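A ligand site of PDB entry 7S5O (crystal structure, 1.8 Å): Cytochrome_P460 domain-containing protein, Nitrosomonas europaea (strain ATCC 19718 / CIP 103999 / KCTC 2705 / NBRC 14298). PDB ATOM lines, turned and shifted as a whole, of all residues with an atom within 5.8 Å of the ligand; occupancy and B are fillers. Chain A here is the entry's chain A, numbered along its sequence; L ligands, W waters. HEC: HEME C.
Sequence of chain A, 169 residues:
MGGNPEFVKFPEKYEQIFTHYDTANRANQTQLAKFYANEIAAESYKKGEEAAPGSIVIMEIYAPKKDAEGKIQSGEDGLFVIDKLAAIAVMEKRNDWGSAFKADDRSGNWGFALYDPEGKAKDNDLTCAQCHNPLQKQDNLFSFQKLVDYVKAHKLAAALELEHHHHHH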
ATOM      1  N   GLY A   2       2.324  16.806 -32.426  1.00  0.00           N
ATOM      2  CA  GLY A   2       0.901  16.867 -32.702  1.00  0.00           C
ATOM      3  C   GLY A   2       0.332  18.217 -32.329  1.00  0.00           C
ATOM      4  O   GLY A   2       0.756  18.850 -31.355  1.00  0.00           O
ATOM      5  N   GLY A   3      -0.620  18.685 -33.123  1.00  0.00           N
ATOM      6  CA  GLY A   3      -1.131  20.031 -32.952  1.00  0.00           C
ATOM      7  C   GLY A   3      -0.252  21.067 -33.624  1.00  0.00           C
ATOM      8  O   GLY A   3       0.781  20.762 -34.215  1.00  0.00           O
ATOM      9  N   TYR A  21     -16.775  24.690 -17.379  1.00  0.00           N
ATOM     10  CA  TYR A  21     -18.094  24.103 -17.561  1.00  0.00           C
ATOM     11  C   TYR A  21     -18.186  22.629 -17.175  1.00  0.00           C
ATOM     12  O   TYR A  21     -19.303  22.113 -17.082  1.00  0.00           O
ATOM     13  CB  TYR A  21     -18.595  24.297 -19.000  1.00  0.00           C
ATOM     14  CG  TYR A  21     -17.827  23.586 -20.108  1.00  0.00           C
ATOM     15  CD1 TYR A  21     -16.771  24.215 -20.763  1.00  0.00           C
ATOM     16  CD2 TYR A  21     -18.198  22.311 -20.524  1.00  0.00           C
ATOM     17  CE1 TYR A  21     -16.081  23.580 -21.790  1.00  0.00           C
ATOM     18  CE2 TYR A  21     -17.511  21.663 -21.553  1.00  0.00           C
ATOM     19  CZ  TYR A  21     -16.469  22.301 -22.180  1.00  0.00           C
ATOM     20  OH  TYR A  21     -15.785  21.675 -23.199  1.00  0.00           O
ATOM     21  N   ASN A  25     -13.492  12.487 -15.162  1.00  0.00           N
ATOM     22  CA  ASN A  25     -12.431  11.579 -15.567  1.00  0.00           C
ATOM     23  C   ASN A  25     -12.399  11.490 -17.076  1.00  0.00           C
ATOM     24  O   ASN A  25     -13.447  11.489 -17.722  1.00  0.00           O
ATOM     25  CB  ASN A  25     -12.642  10.179 -14.988  1.00  0.00           C
ATOM     26  CG  ASN A  25     -12.566  10.132 -13.466  1.00  0.00           C
ATOM     27  OD1 ASN A  25     -11.985  11.007 -12.825  1.00  0.00           O
ATOM     28  ND2 ASN A  25     -13.156   9.093 -12.888  1.00  0.00           N
ATOM     29  N   ARG A  26     -11.201  11.432 -17.656  1.00  0.00           N
ATOM     30  CA  ARG A  26     -11.134  11.203 -19.090  1.00  0.00           C
ATOM     31  C   ARG A  26     -11.552   9.773 -19.402  1.00  0.00           C
ATOM     32  O   ARG A  26     -11.446   8.877 -18.563  1.00  0.00           O
ATOM     33  CB  ARG A  26      -9.717  11.461 -19.612  1.00  0.00           C
ATOM     34  CG  ARG A  26      -9.246  12.920 -19.420  1.00  0.00           C
ATOM     35  CD  ARG A  26      -8.071  13.236 -20.337  1.00  0.00           C
ATOM     36  NE  ARG A  26      -8.457  13.166 -21.737  1.00  0.00           N
ATOM     37  CZ  ARG A  26      -7.626  13.117 -22.756  1.00  0.00           C
ATOM     38  NH1 ARG A  26      -6.307  13.122 -22.584  1.00  0.00           N
ATOM     39  NH2 ARG A  26      -8.113  13.057 -23.989  1.00  0.00           N
ATOM     40  N   ALA A  27     -12.010   9.558 -20.633  1.00  0.00           N
ATOM     41  CA  ALA A  27     -12.461   8.249 -21.072  1.00  0.00           C
ATOM     42  C   ALA A  27     -11.348   7.202 -21.044  1.00  0.00           C
ATOM     43  O   ALA A  27     -11.633   6.010 -20.958  1.00  0.00           O
ATOM     44  CB  ALA A  27     -13.064   8.330 -22.466  1.00  0.00           C
ATOM     45  N   ASN A  28     -10.081   7.629 -21.113  1.00  0.00           N
ATOM     46  CA  ASN A  28      -8.955   6.705 -21.000  1.00  0.00           C
ATOM     47  C   ASN A  28      -8.842   6.110 -19.603  1.00  0.00           C
ATOM     48  O   ASN A  28      -8.080   5.147 -19.417  1.00  0.00           O
ATOM     49  CB  ASN A  28      -7.647   7.392 -21.405  1.00  0.00           C
ATOM     50  CG  ASN A  28      -7.308   8.633 -20.550  1.00  0.00           C
ATOM     51  OD1 ASN A  28      -7.702   8.738 -19.386  1.00  0.00           O
ATOM     52  ND2 ASN A  28      -6.560   9.568 -21.143  1.00  0.00           N
ATOM     53  N   ALA A  33      -9.953  15.456 -16.237  1.00  0.00           N
ATOM     54  CA  ALA A  33     -10.000  16.617 -17.105  1.00  0.00           C
ATOM     55  C   ALA A  33     -10.898  17.687 -16.510  1.00  0.00           C
ATOM     56  O   ALA A  33     -11.908  17.377 -15.859  1.00  0.00           O
ATOM     57  CB  ALA A  33     -10.506  16.235 -18.503  1.00  0.00           C
ATOM     58  N   PHE A  35     -12.725  21.319 -18.063  1.00  0.00           N
ATOM     59  CA  PHE A  35     -13.064  21.856 -19.378  1.00  0.00           C
ATOM     60  C   PHE A  35     -13.460  23.312 -19.249  1.00  0.00           C
ATOM     61  O   PHE A  35     -14.219  23.687 -18.340  1.00  0.00           O
ATOM     62  CB  PHE A  35     -14.217  21.065 -19.998  1.00  0.00           C
ATOM     63  CG  PHE A  35     -13.927  19.597 -20.147  1.00  0.00           C
ATOM     64  CD1 PHE A  35     -14.048  18.736 -19.073  1.00  0.00           C
ATOM     65  CD2 PHE A  35     -13.520  19.101 -21.373  1.00  0.00           C
ATOM     66  CE1 PHE A  35     -13.764  17.380 -19.215  1.00  0.00           C
ATOM     67  CE2 PHE A  35     -13.237  17.753 -21.527  1.00  0.00           C
ATOM     68  CZ  PHE A  35     -13.366  16.887 -20.455  1.00  0.00           C
ATOM     69  N   VAL A  57     -11.911  26.445 -26.710  1.00  0.00           N
ATOM     70  CA  VAL A  57     -12.270  25.473 -25.702  1.00  0.00           C
ATOM     71  C   VAL A  57     -10.973  24.837 -25.212  1.00  0.00           C
ATOM     72  O   VAL A  57     -10.086  24.522 -26.022  1.00  0.00           O
ATOM     73  CB  VAL A  57     -13.239  24.411 -26.264  1.00  0.00           C
ATOM     74  CG1 VAL A  57     -13.466  23.268 -25.256  1.00  0.00           C
ATOM     75  CG2 VAL A  57     -14.573  25.072 -26.630  1.00  0.00           C
ATOM     76  N   ILE A  58     -10.850  24.665 -23.903  1.00  0.00           N
ATOM     77  CA  ILE A  58      -9.630  24.169 -23.292  1.00  0.00           C
ATOM     78  C   ILE A  58      -9.952  22.966 -22.415  1.00  0.00           C
ATOM     79  O   ILE A  58     -10.946  22.949 -21.692  1.00  0.00           O
ATOM     80  CB  ILE A  58      -8.952  25.275 -22.451  1.00  0.00           C
ATOM     81  CG1 ILE A  58      -8.424  26.348 -23.381  1.00  0.00           C
ATOM     82  CG2 ILE A  58      -7.851  24.685 -21.560  1.00  0.00           C
ATOM     83  CD1 ILE A  58      -8.042  27.577 -22.659  1.00  0.00           C
ATOM     84  N   MET A  59      -9.100  21.949 -22.484  1.00  0.00           N
ATOM     85  CA  MET A  59      -9.144  20.832 -21.549  1.00  0.00           C
ATOM     86  C   MET A  59      -7.831  20.808 -20.784  1.00  0.00           C
ATOM     87  O   MET A  59      -6.773  20.539 -21.369  1.00  0.00           O
ATOM     88  CB  MET A  59      -9.392  19.512 -22.272  1.00  0.00           C
ATOM     89  CG  MET A  59      -9.339  18.308 -21.339  1.00  0.00           C
ATOM     90  SD  MET A  59      -9.733  16.766 -22.194  1.00  0.00           S
ATOM     91  CE  MET A  59      -8.384  16.637 -23.385  1.00  0.00           C
ATOM     92  N   ALA A  89      -4.739  21.333 -23.244  1.00  0.00           N
ATOM     93  CA  ALA A  89      -5.100  21.129 -24.635  1.00  0.00           C
ATOM     94  C   ALA A  89      -6.056  22.232 -25.087  1.00  0.00           C
ATOM     95  O   ALA A  89      -6.960  22.616 -24.356  1.00  0.00           O
ATOM     96  CB  ALA A  89      -5.751  19.750 -24.807  1.00  0.00           C
ATOM     97  N   VAL A  90      -5.844  22.729 -26.305  1.00  0.00           N
ATOM     98  CA  VAL A  90      -6.520  23.923 -26.804  1.00  0.00           C
ATOM     99  C   VAL A  90      -7.122  23.633 -28.169  1.00  0.00           C
ATOM    100  O   VAL A  90      -6.439  23.109 -29.056  1.00  0.00           O
ATOM    101  CB  VAL A  90      -5.554  25.124 -26.892  1.00  0.00           C
ATOM    102  CG1 VAL A  90      -6.316  26.390 -27.312  1.00  0.00           C
ATOM    103  CG2 VAL A  90      -4.793  25.350 -25.583  1.00  0.00           C
ATOM    104  N   MET A  91      -8.378  24.001 -28.351  1.00  0.00           N
ATOM    105  CA  MET A  91      -9.048  24.028 -29.648  1.00  0.00           C
ATOM    106  C   MET A  91      -9.505  25.446 -29.901  1.00  0.00           C
ATOM    107  O   MET A  91     -10.118  26.061 -29.027  1.00  0.00           O
ATOM    108  CB  MET A  91     -10.242  23.078 -29.673  1.00  0.00           C
ATOM    109  CG  MET A  91      -9.808  21.629 -29.739  1.00  0.00           C
ATOM    110  SD  MET A  91     -11.176  20.495 -29.572  1.00  0.00           S
ATOM    111  CE  MET A  91     -11.992  20.716 -31.164  1.00  0.00           C
ATOM    112  N   PHE A 112      -5.812  22.864 -33.325  1.00  0.00           N
ATOM    113  CA  PHE A 112      -5.436  22.196 -32.090  1.00  0.00           C
ATOM    114  C   PHE A 112      -4.037  22.604 -31.663  1.00  0.00           C
ATOM    115  O   PHE A 112      -3.185  22.833 -32.515  1.00  0.00           O
ATOM    116  CB  PHE A 112      -5.436  20.665 -32.259  1.00  0.00           C
ATOM    117  CG  PHE A 112      -6.784  20.065 -32.564  1.00  0.00           C
ATOM    118  CD1 PHE A 112      -7.223  19.924 -33.885  1.00  0.00           C
ATOM    119  CD2 PHE A 112      -7.586  19.583 -31.548  1.00  0.00           C
ATOM    120  CE1 PHE A 112      -8.469  19.337 -34.161  1.00  0.00           C
ATOM    121  CE2 PHE A 112      -8.807  19.009 -31.816  1.00  0.00           C
ATOM    122  CZ  PHE A 112      -9.247  18.882 -33.117  1.00  0.00           C
ATOM    123  N   ALA A 113      -3.787  22.646 -30.353  1.00  0.00           N
ATOM    124  CA  ALA A 113      -2.421  22.697 -29.846  1.00  0.00           C
ATOM    125  C   ALA A 113      -2.393  22.154 -28.422  1.00  0.00           C
ATOM    126  O   ALA A 113      -3.357  22.318 -27.662  1.00  0.00           O
ATOM    127  CB  ALA A 113      -1.848  24.126 -29.874  1.00  0.00           C
ATOM    128  N   LEU A 114      -1.288  21.509 -28.070  1.00  0.00           N
ATOM    129  CA  LEU A 114      -1.086  20.950 -26.732  1.00  0.00           C
ATOM    130  C   LEU A 114       0.057  21.689 -26.052  1.00  0.00           C
ATOM    131  O   LEU A 114       1.146  21.794 -26.614  1.00  0.00           O
ATOM    132  CB  LEU A 114      -0.767  19.454 -26.799  1.00  0.00           C
ATOM    133  CG  LEU A 114      -0.684  18.745 -25.450  1.00  0.00           C
ATOM    134  CD1 LEU A 114      -2.061  18.697 -24.816  1.00  0.00           C
ATOM    135  CD2 LEU A 114      -0.112  17.359 -25.634  1.00  0.00           C
ATOM    136  N   ASN A 124       4.478  15.703 -28.338  1.00  0.00           N
ATOM    137  CA  ASN A 124       3.494  14.636 -28.414  1.00  0.00           C
ATOM    138  C   ASN A 124       3.429  14.166 -29.861  1.00  0.00           C
ATOM    139  O   ASN A 124       3.848  14.878 -30.774  1.00  0.00           O
ATOM    140  CB  ASN A 124       2.127  15.112 -27.944  1.00  0.00           C
ATOM    141  CG  ASN A 124       1.451  15.993 -28.956  1.00  0.00           C
ATOM    142  OD1 ASN A 124       0.678  15.511 -29.785  1.00  0.00           O
ATOM    143  ND2 ASN A 124       1.759  17.296 -28.923  1.00  0.00           N
ATOM    144  N   LEU A 126       0.376  12.886 -31.071  1.00  0.00           N
ATOM    145  CA  LEU A 126      -1.059  12.672 -31.252  1.00  0.00           C
ATOM    146  C   LEU A 126      -1.545  13.231 -32.590  1.00  0.00           C
ATOM    147  O   LEU A 126      -1.014  14.217 -33.101  1.00  0.00           O
ATOM    148  CB  LEU A 126      -1.842  13.334 -30.117  1.00  0.00           C
ATOM    149  CG  LEU A 126      -1.545  12.753 -28.730  1.00  0.00           C
ATOM    150  CD1 LEU A 126      -2.326  13.516 -27.678  1.00  0.00           C
ATOM    151  CD2 LEU A 126      -1.858  11.263 -28.708  1.00  0.00           C
ATOM    152  N   THR A 127      -2.558  12.580 -33.151  1.00  0.00           N
ATOM    153  CA  THR A 127      -3.197  13.044 -34.385  1.00  0.00           C
ATOM    154  C   THR A 127      -4.532  13.663 -33.980  1.00  0.00           C
ATOM    155  O   THR A 127      -5.595  13.040 -34.077  1.00  0.00           O
ATOM    156  CB  THR A 127      -3.357  11.894 -35.388  1.00  0.00           C
ATOM    157  OG1 THR A 127      -4.029  10.787 -34.760  1.00  0.00           O
ATOM    158  CG2 THR A 127      -1.968  11.413 -35.884  1.00  0.00           C
ATOM    159  N   CYS A 128      -4.470  14.912 -33.507  1.00  0.00           N
ATOM    160  CA  CYS A 128      -5.621  15.543 -32.852  1.00  0.00           C
ATOM    161  C   CYS A 128      -6.847  15.529 -33.767  1.00  0.00           C
ATOM    162  O   CYS A 128      -7.916  15.040 -33.390  1.00  0.00           O
ATOM    163  CB  CYS A 128      -5.332  16.998 -32.463  1.00  0.00           C
ATOM    164  SG  CYS A 128      -3.709  17.338 -31.771  1.00  0.00           S
ATOM    165  N   ALA A 129      -6.696  16.087 -34.973  1.00  0.00           N
ATOM    166  CA  ALA A 129      -7.846  16.234 -35.849  1.00  0.00           C
ATOM    167  C   ALA A 129      -8.418  14.883 -36.238  1.00  0.00           C
ATOM    168  O   ALA A 129      -9.642  14.721 -36.349  1.00  0.00           O
ATOM    169  CB  ALA A 129      -7.448  17.026 -37.102  1.00  0.00           C
ATOM    170  N   CYS A 131      -8.686  12.140 -34.598  1.00  0.00           N
ATOM    171  CA  CYS A 131      -9.559  11.567 -33.569  1.00  0.00           C
ATOM    172  C   CYS A 131     -10.838  12.382 -33.381  1.00  0.00           C
ATOM    173  O   CYS A 131     -11.906  11.810 -33.096  1.00  0.00           O
ATOM    174  CB  CYS A 131      -8.822  11.474 -32.252  1.00  0.00           C
ATOM    175  SG  CYS A 131      -9.701  10.626 -30.938  1.00  0.00           S
ATOM    176  N   HIS A 132     -10.752  13.701 -33.517  1.00  0.00           N
ATOM    177  CA  HIS A 132     -11.931  14.558 -33.394  1.00  0.00           C
ATOM    178  C   HIS A 132     -12.787  14.608 -34.662  1.00  0.00           C
ATOM    179  O   HIS A 132     -13.969  14.937 -34.561  1.00  0.00           O
ATOM    180  CB  HIS A 132     -11.523  15.989 -33.043  1.00  0.00           C
ATOM    181  CG  HIS A 132     -11.142  16.154 -31.604  1.00  0.00           C
ATOM    182  ND1 HIS A 132     -11.942  16.814 -30.702  1.00  0.00           N
ATOM    183  CD2 HIS A 132     -10.039  15.768 -30.924  1.00  0.00           C
ATOM    184  CE1 HIS A 132     -11.357  16.804 -29.513  1.00  0.00           C
ATOM    185  NE2 HIS A 132     -10.197  16.188 -29.635  1.00  0.00           N
ATOM    186  N   ASN A 140     -17.281  18.513 -33.502  1.00  0.00           N
ATOM    187  CA  ASN A 140     -15.969  17.930 -33.217  1.00  0.00           C
ATOM    188  C   ASN A 140     -15.580  18.069 -31.754  1.00  0.00           C
ATOM    189  O   ASN A 140     -14.391  17.967 -31.409  1.00  0.00           O
ATOM    190  CB  ASN A 140     -14.871  18.531 -34.098  1.00  0.00           C
ATOM    191  CG  ASN A 140     -15.171  18.426 -35.567  1.00  0.00           C
ATOM    192  OD1 ASN A 140     -15.490  19.424 -36.230  1.00  0.00           O
ATOM    193  ND2 ASN A 140     -15.087  17.205 -36.113  1.00  0.00           N
ATOM    194  N   LEU A 141     -16.542  18.281 -30.849  1.00  0.00           N
ATOM    195  CA  LEU A 141     -16.284  18.372 -29.412  1.00  0.00           C
ATOM    196  C   LEU A 141     -16.789  17.109 -28.733  1.00  0.00           C
ATOM    197  O   LEU A 141     -17.985  16.819 -28.812  1.00  0.00           O
ATOM    198  CB  LEU A 141     -16.968  19.578 -28.800  1.00  0.00           C
ATOM    199  CG  LEU A 141     -16.442  20.961 -29.163  1.00  0.00           C
ATOM    200  CD1 LEU A 141     -17.115  22.022 -28.295  1.00  0.00           C
ATOM    201  CD2 LEU A 141     -14.938  21.016 -28.991  1.00  0.00           C
ATOM    202  N   PHE A 142     -15.893  16.364 -28.065  1.00  0.00           N
ATOM    203  CA  PHE A 142     -16.369  15.226 -27.275  1.00  0.00           C
ATOM    204  C   PHE A 142     -17.311  15.678 -26.161  1.00  0.00           C
ATOM    205  O   PHE A 142     -18.317  15.022 -25.887  1.00  0.00           O
ATOM    206  CB  PHE A 142     -15.194  14.451 -26.703  1.00  0.00           C
ATOM    207  CG  PHE A 142     -14.456  13.625 -27.724  1.00  0.00           C
ATOM    208  CD1 PHE A 142     -13.466  14.199 -28.500  1.00  0.00           C
ATOM    209  CD2 PHE A 142     -14.773  12.290 -27.915  1.00  0.00           C
ATOM    210  CE1 PHE A 142     -12.795  13.454 -29.448  1.00  0.00           C
ATOM    211  CE2 PHE A 142     -14.103  11.531 -28.873  1.00  0.00           C
ATOM    212  CZ  PHE A 142     -13.133  12.119 -29.646  1.00  0.00           C
ATOM    213  N   SER A 143     -16.991  16.805 -25.517  1.00  0.00           N
ATOM    214  CA  SER A 143     -17.753  17.298 -24.372  1.00  0.00           C
ATOM    215  C   SER A 143     -18.912  18.213 -24.775  1.00  0.00           C
ATOM    216  O   SER A 143     -19.431  18.942 -23.919  1.00  0.00           O
ATOM    217  CB  SER A 143     -16.831  18.030 -23.391  1.00  0.00           C
ATOM    218  OG  SER A 143     -16.172  19.105 -24.033  1.00  0.00           O
ATOM    219  N   PHE A 144     -19.304  18.173 -26.043  1.00  0.00           N
ATOM    220  CA  PHE A 144     -20.412  18.965 -26.596  1.00  0.00           C
ATOM    221  C   PHE A 144     -21.629  19.081 -25.680  1.00  0.00           C
ATOM    222  O   PHE A 144     -22.083  20.196 -25.373  1.00  0.00           O
ATOM    223  CB  PHE A 144     -20.813  18.327 -27.939  1.00  0.00           C
ATOM    224  CG  PHE A 144     -22.008  18.974 -28.608  1.00  0.00           C
ATOM    225  CD1 PHE A 144     -21.844  20.072 -29.424  1.00  0.00           C
ATOM    226  CD2 PHE A 144     -23.279  18.447 -28.444  1.00  0.00           C
ATOM    227  CE1 PHE A 144     -22.925  20.669 -30.060  1.00  0.00           C
ATOM    228  CE2 PHE A 144     -24.369  19.046 -29.051  1.00  0.00           C
ATOM    229  CZ  PHE A 144     -24.194  20.147 -29.875  1.00  0.00           C
HETATM  230 FE   HEC L   1      -8.864  15.680 -27.877  1.00  0.00          FE
HETATM  231  CHA HEC L   1     -11.281  16.464 -25.529  1.00  0.00           C
HETATM  232  CHB HEC L   1      -7.606  18.868 -27.605  1.00  0.00           C
HETATM  233  CHC HEC L   1      -5.992  14.755 -29.623  1.00  0.00           C
HETATM  234  CHD HEC L   1      -9.758  12.383 -27.750  1.00  0.00           C
HETATM  235  NA  HEC L   1      -9.330  17.341 -26.721  1.00  0.00           N
HETATM  236  C1A HEC L   1     -10.483  17.472 -25.984  1.00  0.00           C
HETATM  237  C2A HEC L   1     -10.694  18.874 -25.727  1.00  0.00           C
HETATM  238  C3A HEC L   1      -9.691  19.558 -26.304  1.00  0.00           C
HETATM  239  C4A HEC L   1      -8.800  18.603 -26.935  1.00  0.00           C
HETATM  240  CMA HEC L   1      -9.511  21.098 -26.292  1.00  0.00           C
HETATM  241  CAA HEC L   1     -11.921  19.424 -24.978  1.00  0.00           C
HETATM  242  CBA HEC L   1     -13.045  19.720 -25.995  1.00  0.00           C
HETATM  243  CGA HEC L   1     -13.775  18.428 -26.358  1.00  0.00           C
HETATM  244  O1A HEC L   1     -13.628  17.914 -27.503  1.00  0.00           O
HETATM  245  O2A HEC L   1     -14.504  17.876 -25.506  1.00  0.00           O
HETATM  246  NB  HEC L   1      -7.122  16.625 -28.496  1.00  0.00           N
HETATM  247  C1B HEC L   1      -6.797  17.960 -28.250  1.00  0.00           C
HETATM  248  C2B HEC L   1      -5.452  18.194 -28.762  1.00  0.00           C
HETATM  249  C3B HEC L   1      -5.027  17.062 -29.357  1.00  0.00           C
HETATM  250  C4B HEC L   1      -6.061  16.059 -29.168  1.00  0.00           C
HETATM  251  CMB HEC L   1      -4.768  19.593 -28.705  1.00  0.00           C
HETATM  252  CAB HEC L   1      -3.695  16.783 -30.102  1.00  0.00           C
HETATM  253  CBB HEC L   1      -2.454  17.211 -29.273  1.00  0.00           C
HETATM  254  NC  HEC L   1      -7.975  13.871 -28.513  1.00  0.00           N
HETATM  255  C1C HEC L   1      -6.905  13.757 -29.368  1.00  0.00           C
HETATM  256  C2C HEC L   1      -6.787  12.370 -29.787  1.00  0.00           C
HETATM  257  C3C HEC L   1      -7.930  11.732 -29.397  1.00  0.00           C
HETATM  258  C4C HEC L   1      -8.640  12.662 -28.516  1.00  0.00           C
HETATM  259  CMC HEC L   1      -5.782  11.996 -30.906  1.00  0.00           C
HETATM  260  CAC HEC L   1      -8.444  10.286 -29.716  1.00  0.00           C
HETATM  261  CBC HEC L   1      -7.330   9.226 -29.832  1.00  0.00           C
HETATM  262  ND  HEC L   1     -10.281  14.597 -26.787  1.00  0.00           N
HETATM  263  C1D HEC L   1     -10.444  13.220 -26.892  1.00  0.00           C
HETATM  264  C2D HEC L   1     -11.463  12.797 -25.939  1.00  0.00           C
HETATM  265  C3D HEC L   1     -11.935  14.069 -25.246  1.00  0.00           C
HETATM  266  C4D HEC L   1     -11.152  15.126 -25.831  1.00  0.00           C
HETATM  267  CMD HEC L   1     -12.007  11.374 -25.684  1.00  0.00           C
HETATM  268  CAD HEC L   1     -13.017  14.193 -24.155  1.00  0.00           C
HETATM  269  CBD HEC L   1     -12.407  14.073 -22.748  1.00  0.00           C
HETATM  270  CGD HEC L   1     -12.052  12.626 -22.494  1.00  0.00           C
HETATM  271  O1D HEC L   1     -10.891  12.273 -22.683  1.00  0.00           O
HETATM  272  O2D HEC L   1     -12.952  11.829 -22.103  1.00  0.00           O
HETATM  273  O   HOH W   1      -9.727   9.911 -22.979  1.00  0.00           O
HETATM  274  O   HOH W   2     -15.365  11.347 -23.238  1.00  0.00           O
HETATM  275  O   HOH W   3     -14.397  12.976 -19.908  1.00  0.00           O
HETATM  276  O   HOH W   4      -6.331  12.397 -26.085  1.00  0.00           O
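The side-chain sulfur (SG) of Cys 128 is bonded to a carbon (CAB) of the ligand, 1.8 Å away.
SG of Cys 131 is bonded to CAC of the ligand, 1.8 Å away.
A ring nitrogen (NE2) of His 132 is bound to an iron atom (FE) of the ligand, 2.3 Å away.
O2A of the ligand lies within hydrogen-bond range of N of Ser 143 (2.7 Å).
OG of Ser 143 sits at hydrogen-bond distance from O2A of the ligand (2.5 Å).
NE of Arg 26 lies within salt-bridge range of O1D of the ligand (2.8 Å).
The backbone NH (N) of Phe 142 lies within hydrogen-bond range of an oxygen (O1A) of the ligand, 2.8 Å away.
An oxygen (O2D) of the ligand lies within hydrogen-bond range of the backbone NH (N) of Ala 27 (2.9 Å).
The side-chain sulfur (SG) of Cys 128 is in hydrogen-bond range of the backbone NH (N) of Gly 3, 3.6 Å away.
The side-chain hydroxyl (OG) of Ser 143 sits at hydrogen-bond distance from the side-chain hydroxyl (OH) of Tyr 21.
O of Ala 113 lies within hydrogen-bond range of N of Val 90 (2.9 Å).
O of Met 59 is in hydrogen-bond range of N of Ala 89, at 2.9 Å.
N of Met 91 sits at hydrogen-bond distance from O of Val 57, at 2.9 Å.
N of Leu 126 sits at hydrogen-bond distance from OD1 of Asn 124.
The backbone carbonyl oxygen (O) of Asn 124 lies within hydrogen-bond range of the backbone NH (N) of Gly 2 (3.0 Å).
N of Tyr 21 sits at hydrogen-bond distance from O of Phe 35 (2.9 Å).
Phe 35 touches the ligand.
O of Val 57 touches CMA of the ligand (3.5 Å).
CE of Met 59 touches C1A of the ligand (3.4 Å).
CB of Ala 89 touches CHB of the ligand (3.5 Å).
O of Val 90 touches CMB of the ligand, at 3.9 Å.
Met 91 touches the ligand (CG to CMA, 3.5 Å).
CD2 of Phe 112 touches C1B of the ligand, at 3.8 Å.
O of Ala 113 touches CMB of the ligand (3.2 Å).
CB of Leu 114 touches CBB of the ligand, at 3.7 Å.
Asn 124 touches the ligand.
Leu 126 touches the ligand.
Thr 127 touches the ligand.
Asn 140 touches the ligand.
CA of Leu 141 touches O1A of the ligand (3.3 Å).
Hydrophobic or aromatic side chains within 4 Å of the ligand: Ala 27, Phe 35, Val 57, Met 59, Ala 89, Met 91, Phe 112, Leu 114, Leu 126, His 132, Leu 141 and Phe 142.
21 residues have an atom within 4 Å of the ligand: Arg 26, Ala 27, Phe 35, Val 57, Met 59, Ala 89, Val 90, Met 91, Phe 112, Ala 113, Leu 114, Asn 124, Leu 126, Thr 127, Cys 128, Cys 131, His 132, Asn 140, Leu 141, Phe 142 and Ser 143.
The nearest printed residue that does not touch the ligand is Gly 2 (4.2 Å).
Water W1 lies within hydrogen-bond range of O1D of the ligand (2.6 Å), N of Asn 28 (3.0 Å) and N of Ala 27 (3.3 Å).
Water W3 bridges the backbone carbonyl oxygen (O) of Asn 25 (2.8 Å) and an oxygen (O2D) of the ligand (2.9 Å).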
